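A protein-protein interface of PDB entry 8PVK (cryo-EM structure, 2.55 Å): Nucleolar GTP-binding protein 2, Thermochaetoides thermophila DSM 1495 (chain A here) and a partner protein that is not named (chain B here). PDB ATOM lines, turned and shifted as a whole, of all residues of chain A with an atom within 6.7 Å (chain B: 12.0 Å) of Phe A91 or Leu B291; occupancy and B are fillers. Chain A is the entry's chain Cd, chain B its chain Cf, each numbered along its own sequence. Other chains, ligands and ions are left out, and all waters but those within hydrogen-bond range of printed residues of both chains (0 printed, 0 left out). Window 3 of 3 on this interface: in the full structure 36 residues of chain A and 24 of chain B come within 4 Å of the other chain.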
ATOM      1  N   ILE A  83     -26.665  31.807  13.517  1.00  0.00           N
ATOM      2  CA  ILE A  83     -27.276  30.503  13.307  1.00  0.00           C
ATOM      3  C   ILE A  83     -27.358  29.795  14.654  1.00  0.00           C
ATOM      4  O   ILE A  83     -26.529  30.012  15.542  1.00  0.00           O
ATOM      5  CB  ILE A  83     -26.499  29.678  12.245  1.00  0.00           C
ATOM      6  CG1 ILE A  83     -27.331  28.492  11.750  1.00  0.00           C
ATOM      7  CG2 ILE A  83     -25.136  29.229  12.762  1.00  0.00           C
ATOM      8  CD1 ILE A  83     -26.789  27.845  10.502  1.00  0.00           C
ATOM      9  N   ASP A  86     -29.716  24.060  16.777  1.00  0.00           N
ATOM     10  CA  ASP A  86     -30.710  23.174  16.175  1.00  0.00           C
ATOM     11  C   ASP A  86     -30.677  23.257  14.654  1.00  0.00           C
ATOM     12  O   ASP A  86     -30.776  22.233  13.963  1.00  0.00           O
ATOM     13  CB  ASP A  86     -32.102  23.520  16.698  1.00  0.00           C
ATOM     14  CG  ASP A  86     -32.275  23.176  18.163  1.00  0.00           C
ATOM     15  OD1 ASP A  86     -31.614  22.226  18.632  1.00  0.00           O
ATOM     16  OD2 ASP A  86     -33.070  23.855  18.845  1.00  0.00           O
ATOM     17  N   THR A  87     -30.529  24.471  14.119  1.00  0.00           N
ATOM     18  CA  THR A  87     -30.388  24.649  12.678  1.00  0.00           C
ATOM     19  C   THR A  87     -29.109  23.995  12.170  1.00  0.00           C
ATOM     20  O   THR A  87     -29.096  23.389  11.090  1.00  0.00           O
ATOM     21  CB  THR A  87     -30.410  26.140  12.341  1.00  0.00           C
ATOM     22  OG1 THR A  87     -31.556  26.749  12.948  1.00  0.00           O
ATOM     23  CG2 THR A  87     -30.487  26.353  10.844  1.00  0.00           C
ATOM     24  N   LEU A  88     -28.026  24.092  12.950  1.00  0.00           N
ATOM     25  CA  LEU A  88     -26.778  23.428  12.583  1.00  0.00           C
ATOM     26  C   LEU A  88     -26.931  21.911  12.562  1.00  0.00           C
ATOM     27  O   LEU A  88     -26.419  21.248  11.656  1.00  0.00           O
ATOM     28  CB  LEU A  88     -25.662  23.841  13.541  1.00  0.00           C
ATOM     29  CG  LEU A  88     -24.947  25.149  13.201  1.00  0.00           C
ATOM     30  CD1 LEU A  88     -23.917  25.492  14.263  1.00  0.00           C
ATOM     31  CD2 LEU A  88     -24.300  25.063  11.828  1.00  0.00           C
ATOM     32  N   GLN A  89     -27.634  21.344  13.551  1.00  0.00           N
ATOM     33  CA  GLN A  89     -27.883  19.902  13.560  1.00  0.00           C
ATOM     34  C   GLN A  89     -28.724  19.469  12.365  1.00  0.00           C
ATOM     35  O   GLN A  89     -28.448  18.431  11.749  1.00  0.00           O
ATOM     36  CB  GLN A  89     -28.569  19.476  14.859  1.00  0.00           C
ATOM     37  CG  GLN A  89     -27.756  19.673  16.122  1.00  0.00           C
ATOM     38  CD  GLN A  89     -26.532  18.782  16.168  1.00  0.00           C
ATOM     39  OE1 GLN A  89     -26.579  17.625  15.754  1.00  0.00           O
ATOM     40  NE2 GLN A  89     -25.433  19.313  16.689  1.00  0.00           N
ATOM     41  N   SER A  90     -29.759  20.247  12.031  1.00  0.00           N
ATOM     42  CA  SER A  90     -30.595  19.916  10.881  1.00  0.00           C
ATOM     43  C   SER A  90     -29.797  19.960   9.583  1.00  0.00           C
ATOM     44  O   SER A  90     -29.929  19.071   8.731  1.00  0.00           O
ATOM     45  CB  SER A  90     -31.789  20.867  10.809  1.00  0.00           C
ATOM     46  OG  SER A  90     -32.575  20.785  11.983  1.00  0.00           O
ATOM     47  N   PHE A  91     -28.945  20.974   9.427  1.00  0.00           N
ATOM     48  CA  PHE A  91     -28.128  21.070   8.223  1.00  0.00           C
ATOM     49  C   PHE A  91     -27.065  19.978   8.165  1.00  0.00           C
ATOM     50  O   PHE A  91     -26.747  19.492   7.077  1.00  0.00           O
ATOM     51  CB  PHE A  91     -27.493  22.456   8.134  1.00  0.00           C
ATOM     52  CG  PHE A  91     -28.419  23.503   7.590  1.00  0.00           C
ATOM     53  CD1 PHE A  91     -29.352  23.178   6.620  1.00  0.00           C
ATOM     54  CD2 PHE A  91     -28.367  24.806   8.054  1.00  0.00           C
ATOM     55  CE1 PHE A  91     -30.212  24.134   6.117  1.00  0.00           C
ATOM     56  CE2 PHE A  91     -29.228  25.767   7.555  1.00  0.00           C
ATOM     57  CZ  PHE A  91     -30.148  25.430   6.584  1.00  0.00           C
ATOM     58  N   ARG A  92     -26.519  19.572   9.315  1.00  0.00           N
ATOM     59  CA  ARG A  92     -25.570  18.460   9.334  1.00  0.00           C
ATOM     60  C   ARG A  92     -26.241  17.145   8.955  1.00  0.00           C
ATOM     61  O   ARG A  92     -25.654  16.332   8.232  1.00  0.00           O
ATOM     62  CB  ARG A  92     -24.911  18.349  10.708  1.00  0.00           C
ATOM     63  CG  ARG A  92     -23.871  19.416  10.982  1.00  0.00           C
ATOM     64  CD  ARG A  92     -23.147  19.152  12.286  1.00  0.00           C
ATOM     65  NE  ARG A  92     -22.425  20.330  12.749  1.00  0.00           N
ATOM     66  CZ  ARG A  92     -22.768  21.050  13.809  1.00  0.00           C
ATOM     67  NH1 ARG A  92     -23.821  20.739  14.543  1.00  0.00           N
ATOM     68  NH2 ARG A  92     -22.032  22.107  14.140  1.00  0.00           N
ATOM     69  N   GLU A  93     -27.470  16.919   9.431  1.00  0.00           N
ATOM     70  CA  GLU A  93     -28.204  15.721   9.028  1.00  0.00           C
ATOM     71  C   GLU A  93     -28.526  15.741   7.537  1.00  0.00           C
ATOM     72  O   GLU A  93     -28.431  14.706   6.863  1.00  0.00           O
ATOM     73  CB  GLU A  93     -29.480  15.581   9.856  1.00  0.00           C
ATOM     74  CG  GLU A  93     -29.235  15.270  11.322  1.00  0.00           C
ATOM     75  CD  GLU A  93     -30.408  15.645  12.204  1.00  0.00           C
ATOM     76  OE1 GLU A  93     -31.382  16.229  11.684  1.00  0.00           O
ATOM     77  OE2 GLU A  93     -30.357  15.357  13.418  1.00  0.00           O
ATOM     78  N   ALA A  94     -28.907  16.911   7.009  1.00  0.00           N
ATOM     79  CA  ALA A  94     -29.167  17.035   5.576  1.00  0.00           C
ATOM     80  C   ALA A  94     -27.907  16.784   4.755  1.00  0.00           C
ATOM     81  O   ALA A  94     -27.962  16.135   3.703  1.00  0.00           O
ATOM     82  CB  ALA A  94     -29.740  18.418   5.270  1.00  0.00           C
ATOM     83  N   MET A  95     -26.763  17.295   5.220  1.00  0.00           N
ATOM     84  CA  MET A  95     -25.487  17.023   4.568  1.00  0.00           C
ATOM     85  C   MET A  95     -25.134  15.542   4.618  1.00  0.00           C
ATOM     86  O   MET A  95     -24.571  15.007   3.656  1.00  0.00           O
ATOM     87  CB  MET A  95     -24.383  17.853   5.228  1.00  0.00           C
ATOM     88  CG  MET A  95     -23.019  17.754   4.564  1.00  0.00           C
ATOM     89  SD  MET A  95     -22.993  18.394   2.881  1.00  0.00           S
ATOM     90  CE  MET A  95     -23.108  20.153   3.193  1.00  0.00           C
ATOM     91  N   ALA A  96     -25.451  14.872   5.730  1.00  0.00           N
ATOM     92  CA  ALA A  96     -25.167  13.446   5.854  1.00  0.00           C
ATOM     93  C   ALA A  96     -26.012  12.621   4.889  1.00  0.00           C
ATOM     94  O   ALA A  96     -25.507  11.691   4.249  1.00  0.00           O
ATOM     95  CB  ALA A  96     -25.397  12.991   7.295  1.00  0.00           C
ATOM     96  N   GLU A  97     -27.303  12.943   4.766  1.00  0.00           N
ATOM     97  CA  GLU A  97     -28.194  12.162   3.911  1.00  0.00           C
ATOM     98  C   GLU A  97     -28.317  12.731   2.500  1.00  0.00           C
ATOM     99  O   GLU A  97     -29.177  12.282   1.731  1.00  0.00           O
ATOM    100  CB  GLU A  97     -29.579  12.028   4.547  1.00  0.00           C
ATOM    101  CG  GLU A  97     -30.350  13.328   4.677  1.00  0.00           C
ATOM    102  CD  GLU A  97     -31.688  13.149   5.371  1.00  0.00           C
ATOM    103  OE1 GLU A  97     -32.009  12.010   5.774  1.00  0.00           O
ATOM    104  OE2 GLU A  97     -32.422  14.150   5.509  1.00  0.00           O
ATOM    105  N   ASN A 110     -27.190  28.302  -1.169  1.00  0.00           N
ATOM    106  CA  ASN A 110     -27.595  28.909   0.091  1.00  0.00           C
ATOM    107  C   ASN A 110     -26.359  29.343   0.868  1.00  0.00           C
ATOM    108  O   ASN A 110     -25.442  28.544   1.083  1.00  0.00           O
ATOM    109  CB  ASN A 110     -28.427  27.930   0.918  1.00  0.00           C
ATOM    110  CG  ASN A 110     -29.201  28.614   2.023  1.00  0.00           C
ATOM    111  OD1 ASN A 110     -29.362  29.832   2.020  1.00  0.00           O
ATOM    112  ND2 ASN A 110     -29.683  27.831   2.979  1.00  0.00           N
ATOM    113  N   LEU A 112     -24.312  29.680   3.774  1.00  0.00           N
ATOM    114  CA  LEU A 112     -24.326  28.937   5.025  1.00  0.00           C
ATOM    115  C   LEU A 112     -22.895  28.710   5.485  1.00  0.00           C
ATOM    116  O   LEU A 112     -21.971  28.752   4.664  1.00  0.00           O
ATOM    117  CB  LEU A 112     -25.054  27.595   4.853  1.00  0.00           C
ATOM    118  CG  LEU A 112     -26.579  27.597   4.838  1.00  0.00           C
ATOM    119  CD1 LEU A 112     -27.105  26.181   4.713  1.00  0.00           C
ATOM    120  CD2 LEU A 112     -27.105  28.258   6.097  1.00  0.00           C
ATOM    121  N   PRO A 113     -22.673  28.491   6.788  1.00  0.00           N
ATOM    122  CA  PRO A 113     -21.326  28.119   7.249  1.00  0.00           C
ATOM    123  C   PRO A 113     -20.973  26.664   6.961  1.00  0.00           C
ATOM    124  O   PRO A 113     -21.160  25.787   7.812  1.00  0.00           O
ATOM    125  CB  PRO A 113     -21.380  28.403   8.754  1.00  0.00           C
ATOM    126  CG  PRO A 113     -22.816  28.314   9.109  1.00  0.00           C
ATOM    127  CD  PRO A 113     -23.584  28.777   7.911  1.00  0.00           C
ATOM    128  N   ILE A 117     -20.903  23.088   8.996  1.00  0.00           N
ATOM    129  CA  ILE A 117     -21.918  22.133   8.564  1.00  0.00           C
ATOM    130  C   ILE A 117     -21.297  20.829   8.066  1.00  0.00           C
ATOM    131  O   ILE A 117     -21.702  19.745   8.489  1.00  0.00           O
ATOM    132  CB  ILE A 117     -22.849  22.753   7.496  1.00  0.00           C
ATOM    133  CG1 ILE A 117     -23.699  23.861   8.119  1.00  0.00           C
ATOM    134  CG2 ILE A 117     -23.746  21.696   6.874  1.00  0.00           C
ATOM    135  CD1 ILE A 117     -24.508  24.642   7.119  1.00  0.00           C
ATOM    136  N   ARG A 118     -20.313  20.911   7.172  1.00  0.00           N
ATOM    137  CA  ARG A 118     -19.760  19.696   6.585  1.00  0.00           C
ATOM    138  C   ARG A 118     -18.906  18.942   7.599  1.00  0.00           C
ATOM    139  O   ARG A 118     -18.401  19.509   8.572  1.00  0.00           O
ATOM    140  CB  ARG A 118     -18.928  20.009   5.338  1.00  0.00           C
ATOM    141  CG  ARG A 118     -17.542  20.568   5.612  1.00  0.00           C
ATOM    142  CD  ARG A 118     -16.779  20.843   4.325  1.00  0.00           C
ATOM    143  NE  ARG A 118     -17.377  21.907   3.527  1.00  0.00           N
ATOM    144  CZ  ARG A 118     -18.029  21.712   2.389  1.00  0.00           C
ATOM    145  NH1 ARG A 118     -18.201  20.498   1.891  1.00  0.00           N
ATOM    146  NH2 ARG A 118     -18.517  22.759   1.731  1.00  0.00           N
ATOM    147  N   GLU B 281     -45.095  30.041   0.181  1.00  0.00           N
ATOM    148  CA  GLU B 281     -44.445  30.226  -1.106  1.00  0.00           C
ATOM    149  C   GLU B 281     -45.353  29.789  -2.249  1.00  0.00           C
ATOM    150  O   GLU B 281     -46.275  28.988  -2.074  1.00  0.00           O
ATOM    151  CB  GLU B 281     -43.129  29.446  -1.159  1.00  0.00           C
ATOM    152  CG  GLU B 281     -43.291  27.933  -1.209  1.00  0.00           C
ATOM    153  CD  GLU B 281     -43.327  27.292   0.167  1.00  0.00           C
ATOM    154  OE1 GLU B 281     -43.491  28.023   1.167  1.00  0.00           O
ATOM    155  OE2 GLU B 281     -43.194  26.053   0.248  1.00  0.00           O
ATOM    156  N   ILE B 287     -38.948  23.818 -10.024  1.00  0.00           N
ATOM    157  CA  ILE B 287     -38.142  24.550  -9.056  1.00  0.00           C
ATOM    158  C   ILE B 287     -38.497  24.038  -7.670  1.00  0.00           C
ATOM    159  O   ILE B 287     -39.677  23.989  -7.307  1.00  0.00           O
ATOM    160  CB  ILE B 287     -38.376  26.070  -9.140  1.00  0.00           C
ATOM    161  CG1 ILE B 287     -38.269  26.561 -10.583  1.00  0.00           C
ATOM    162  CG2 ILE B 287     -37.395  26.811  -8.244  1.00  0.00           C
ATOM    163  CD1 ILE B 287     -36.886  26.462 -11.152  1.00  0.00           C
ATOM    164  N   SER B 288     -37.482  23.661  -6.897  1.00  0.00           N
ATOM    165  CA  SER B 288     -37.695  23.228  -5.526  1.00  0.00           C
ATOM    166  C   SER B 288     -36.561  23.760  -4.663  1.00  0.00           C
ATOM    167  O   SER B 288     -35.609  24.367  -5.157  1.00  0.00           O
ATOM    168  CB  SER B 288     -37.797  21.700  -5.433  1.00  0.00           C
ATOM    169  OG  SER B 288     -36.537  21.090  -5.638  1.00  0.00           O
ATOM    170  N   MET B 289     -36.674  23.543  -3.359  1.00  0.00           N
ATOM    171  CA  MET B 289     -35.625  23.875  -2.408  1.00  0.00           C
ATOM    172  C   MET B 289     -35.228  22.605  -1.674  1.00  0.00           C
ATOM    173  O   MET B 289     -36.089  21.913  -1.121  1.00  0.00           O
ATOM    174  CB  MET B 289     -36.096  24.943  -1.420  1.00  0.00           C
ATOM    175  CG  MET B 289     -35.040  25.383  -0.426  1.00  0.00           C
ATOM    176  SD  MET B 289     -35.650  26.657   0.691  1.00  0.00           S
ATOM    177  CE  MET B 289     -36.763  25.703   1.716  1.00  0.00           C
ATOM    178  N   ASP B 290     -33.935  22.294  -1.667  1.00  0.00           N
ATOM    179  CA  ASP B 290     -33.493  21.062  -1.024  1.00  0.00           C
ATOM    180  C   ASP B 290     -33.403  21.283   0.487  1.00  0.00           C
ATOM    181  O   ASP B 290     -33.718  22.359   1.003  1.00  0.00           O
ATOM    182  CB  ASP B 290     -32.185  20.564  -1.642  1.00  0.00           C
ATOM    183  CG  ASP B 290     -30.997  21.457  -1.333  1.00  0.00           C
ATOM    184  OD1 ASP B 290     -31.189  22.629  -0.957  1.00  0.00           O
ATOM    185  OD2 ASP B 290     -29.851  20.978  -1.472  1.00  0.00           O
ATOM    186  N   LEU B 291     -32.959  20.265   1.220  1.00  0.00           N
ATOM    187  CA  LEU B 291     -32.897  20.367   2.672  1.00  0.00           C
ATOM    188  C   LEU B 291     -31.722  21.202   3.163  1.00  0.00           C
ATOM    189  O   LEU B 291     -31.664  21.513   4.357  1.00  0.00           O
ATOM    190  CB  LEU B 291     -32.843  18.971   3.295  1.00  0.00           C
ATOM    191  CG  LEU B 291     -34.174  18.216   3.284  1.00  0.00           C
ATOM    192  CD1 LEU B 291     -34.032  16.858   3.948  1.00  0.00           C
ATOM    193  CD2 LEU B 291     -35.265  19.038   3.956  1.00  0.00           C
ATOM    194  N   LEU B 292     -30.791  21.567   2.286  1.00  0.00           N
ATOM    195  CA  LEU B 292     -29.724  22.498   2.622  1.00  0.00           C
ATOM    196  C   LEU B 292     -30.041  23.930   2.214  1.00  0.00           C
ATOM    197  O   LEU B 292     -29.193  24.810   2.385  1.00  0.00           O
ATOM    198  CB  LEU B 292     -28.409  22.056   1.974  1.00  0.00           C
ATOM    199  CG  LEU B 292     -27.670  20.919   2.679  1.00  0.00           C
ATOM    200  CD1 LEU B 292     -26.594  20.352   1.775  1.00  0.00           C
ATOM    201  CD2 LEU B 292     -27.071  21.401   3.990  1.00  0.00           C
ATOM    202  N   GLY B 293     -31.233  24.181   1.679  1.00  0.00           N
ATOM    203  CA  GLY B 293     -31.644  25.516   1.303  1.00  0.00           C
ATOM    204  C   GLY B 293     -31.271  25.949  -0.098  1.00  0.00           C
ATOM    205  O   GLY B 293     -31.568  27.090  -0.472  1.00  0.00           O
ATOM    206  N   ASP B 294     -30.630  25.087  -0.881  1.00  0.00           N
ATOM    207  CA  ASP B 294     -30.285  25.426  -2.254  1.00  0.00           C
ATOM    208  C   ASP B 294     -31.509  25.322  -3.153  1.00  0.00           C
ATOM    209  O   ASP B 294     -32.354  24.433  -2.983  1.00  0.00           O
ATOM    210  CB  ASP B 294     -29.187  24.503  -2.780  1.00  0.00           C
ATOM    211  CG  ASP B 294     -27.946  24.516  -1.917  1.00  0.00           C
ATOM    212  OD1 ASP B 294     -27.795  25.447  -1.102  1.00  0.00           O
ATOM    213  OD2 ASP B 294     -27.116  23.594  -2.056  1.00  0.00           O
ATOM    214  N   LYS B 295     -31.597  26.241  -4.113  1.00  0.00           N
ATOM    215  CA  LYS B 295     -32.608  26.167  -5.156  1.00  0.00           C
ATOM    216  C   LYS B 295     -32.185  25.135  -6.193  1.00  0.00           C
ATOM    217  O   LYS B 295     -31.071  25.193  -6.720  1.00  0.00           O
ATOM    218  CB  LYS B 295     -32.805  27.533  -5.811  1.00  0.00           C
ATOM    219  CG  LYS B 295     -34.029  27.622  -6.704  1.00  0.00           C
ATOM    220  CD  LYS B 295     -34.131  28.981  -7.376  1.00  0.00           C
ATOM    221  CE  LYS B 295     -34.284  30.096  -6.356  1.00  0.00           C
ATOM    222  NZ  LYS B 295     -34.362  31.432  -7.009  1.00  0.00           N
ATOM    223  N   ILE B 296     -33.075  24.191  -6.480  1.00  0.00           N
ATOM    224  CA  ILE B 296     -32.781  23.043  -7.326  1.00  0.00           C
ATOM    225  C   ILE B 296     -33.739  23.057  -8.509  1.00  0.00           C
ATOM    226  O   ILE B 296     -34.956  23.199  -8.329  1.00  0.00           O
ATOM    227  CB  ILE B 296     -32.895  21.723  -6.539  1.00  0.00           C
ATOM    228  CG1 ILE B 296     -31.951  21.737  -5.336  1.00  0.00           C
ATOM    229  CG2 ILE B 296     -32.592  20.536  -7.426  1.00  0.00           C
ATOM    230  CD1 ILE B 296     -30.493  21.913  -5.705  1.00  0.00           C
ATOM    231  N   GLY B 297     -33.187  22.917  -9.712  1.00  0.00           N
ATOM    232  CA  GLY B 297     -33.968  22.863 -10.933  1.00  0.00           C
ATOM    233  C   GLY B 297     -33.988  21.459 -11.505  1.00  0.00           C
ATOM    234  O   GLY B 297     -33.011  20.715 -11.393  1.00  0.00           O
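Of the 12 printed residues of chain B, 4 touch a printed residue of chain A. Of the 18 printed residues of chain A, 6 touch a printed residue of chain B. Among the printed residues, no Asp or Glu carboxylate lies within 4 Å of a Lys or Arg side-chain nitrogen of the other chain.
OD1 of Asp B290 lies close to N of Leu B292 (3.4 Å). The side-chain carboxylate of Asp B290 sits at hydrogen-bond distance from the backbone NH of Gly B293 (3.1 Å). The backbone NH (N) of Asp B294 sits at hydrogen-bond distance from the side-chain carboxylate (OD1) of Asp B290.
Phe A91 touches just these residues of chain B: Leu B291 (3.5 Å) and Leu B292 (3.6 Å). Of chain A, only Phe A91 (3.5 Å), Ala A94 (3.7 Å) and Glu A97 (3.5 Å) come within 4 Å of Leu B291. No residue of chain B comes within 4 Å of Leu A88. No residue of chain B comes within 4 Å of Ser A90. Met A95 touches one residue of chain B. No residue of chain B comes within 4 Å of Pro A113. No residue of chain B comes within 4 Å of Ile A117. Printed residues of chain B within 4 Å of Asn A110: Leu B292, Gly B293 and Asp B294. Of the printed residues of chain A, Leu B292 touches Phe A91, Met A95, Asn A110 and Leu A112. Of the printed residues of chain B, Leu A112 touches Leu B292 (3.4 Å). Printed residues of chain A within 4 Å of Gly B293: Asn A110 (3.5 Å). Of the printed residues of chain A, Asp B294 touches Asn A110. Lys B295 touches none of the printed residues of chain A. Asp A86 touches none of the printed residues of chain B. The nearest residue of chain B that does not touch Phe A91 is Gly B293 (4.6 Å). The nearest residue of chain A that does not touch Leu B291 is Ser A90 (5.3 Å). The nearest printed residue of chain B that does not touch Leu A112 is Gly B293 (5.5 Å).
Among the printed residues, merely in contact across the chains: Phe A91 with Leu B291 (3.5 Å), Phe A91 with Leu B292 (3.6 Å), Ala A94 with Leu B291 (3.7 Å), Met A95 with Leu B292 (3.8 Å), Glu A97 with Leu B291 (3.5 Å), Asn A110 with Gly B293 (3.5 Å) and Leu A112 with Leu B292 (3.4 Å).
ND2 of Asn A110 is in hydrogen-bond range of O of Leu B292 (3.1 Å). The backbone NH (N) of Asn A110 sits at hydrogen-bond distance from the side-chain carboxylate (OD1) of Asp B294.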
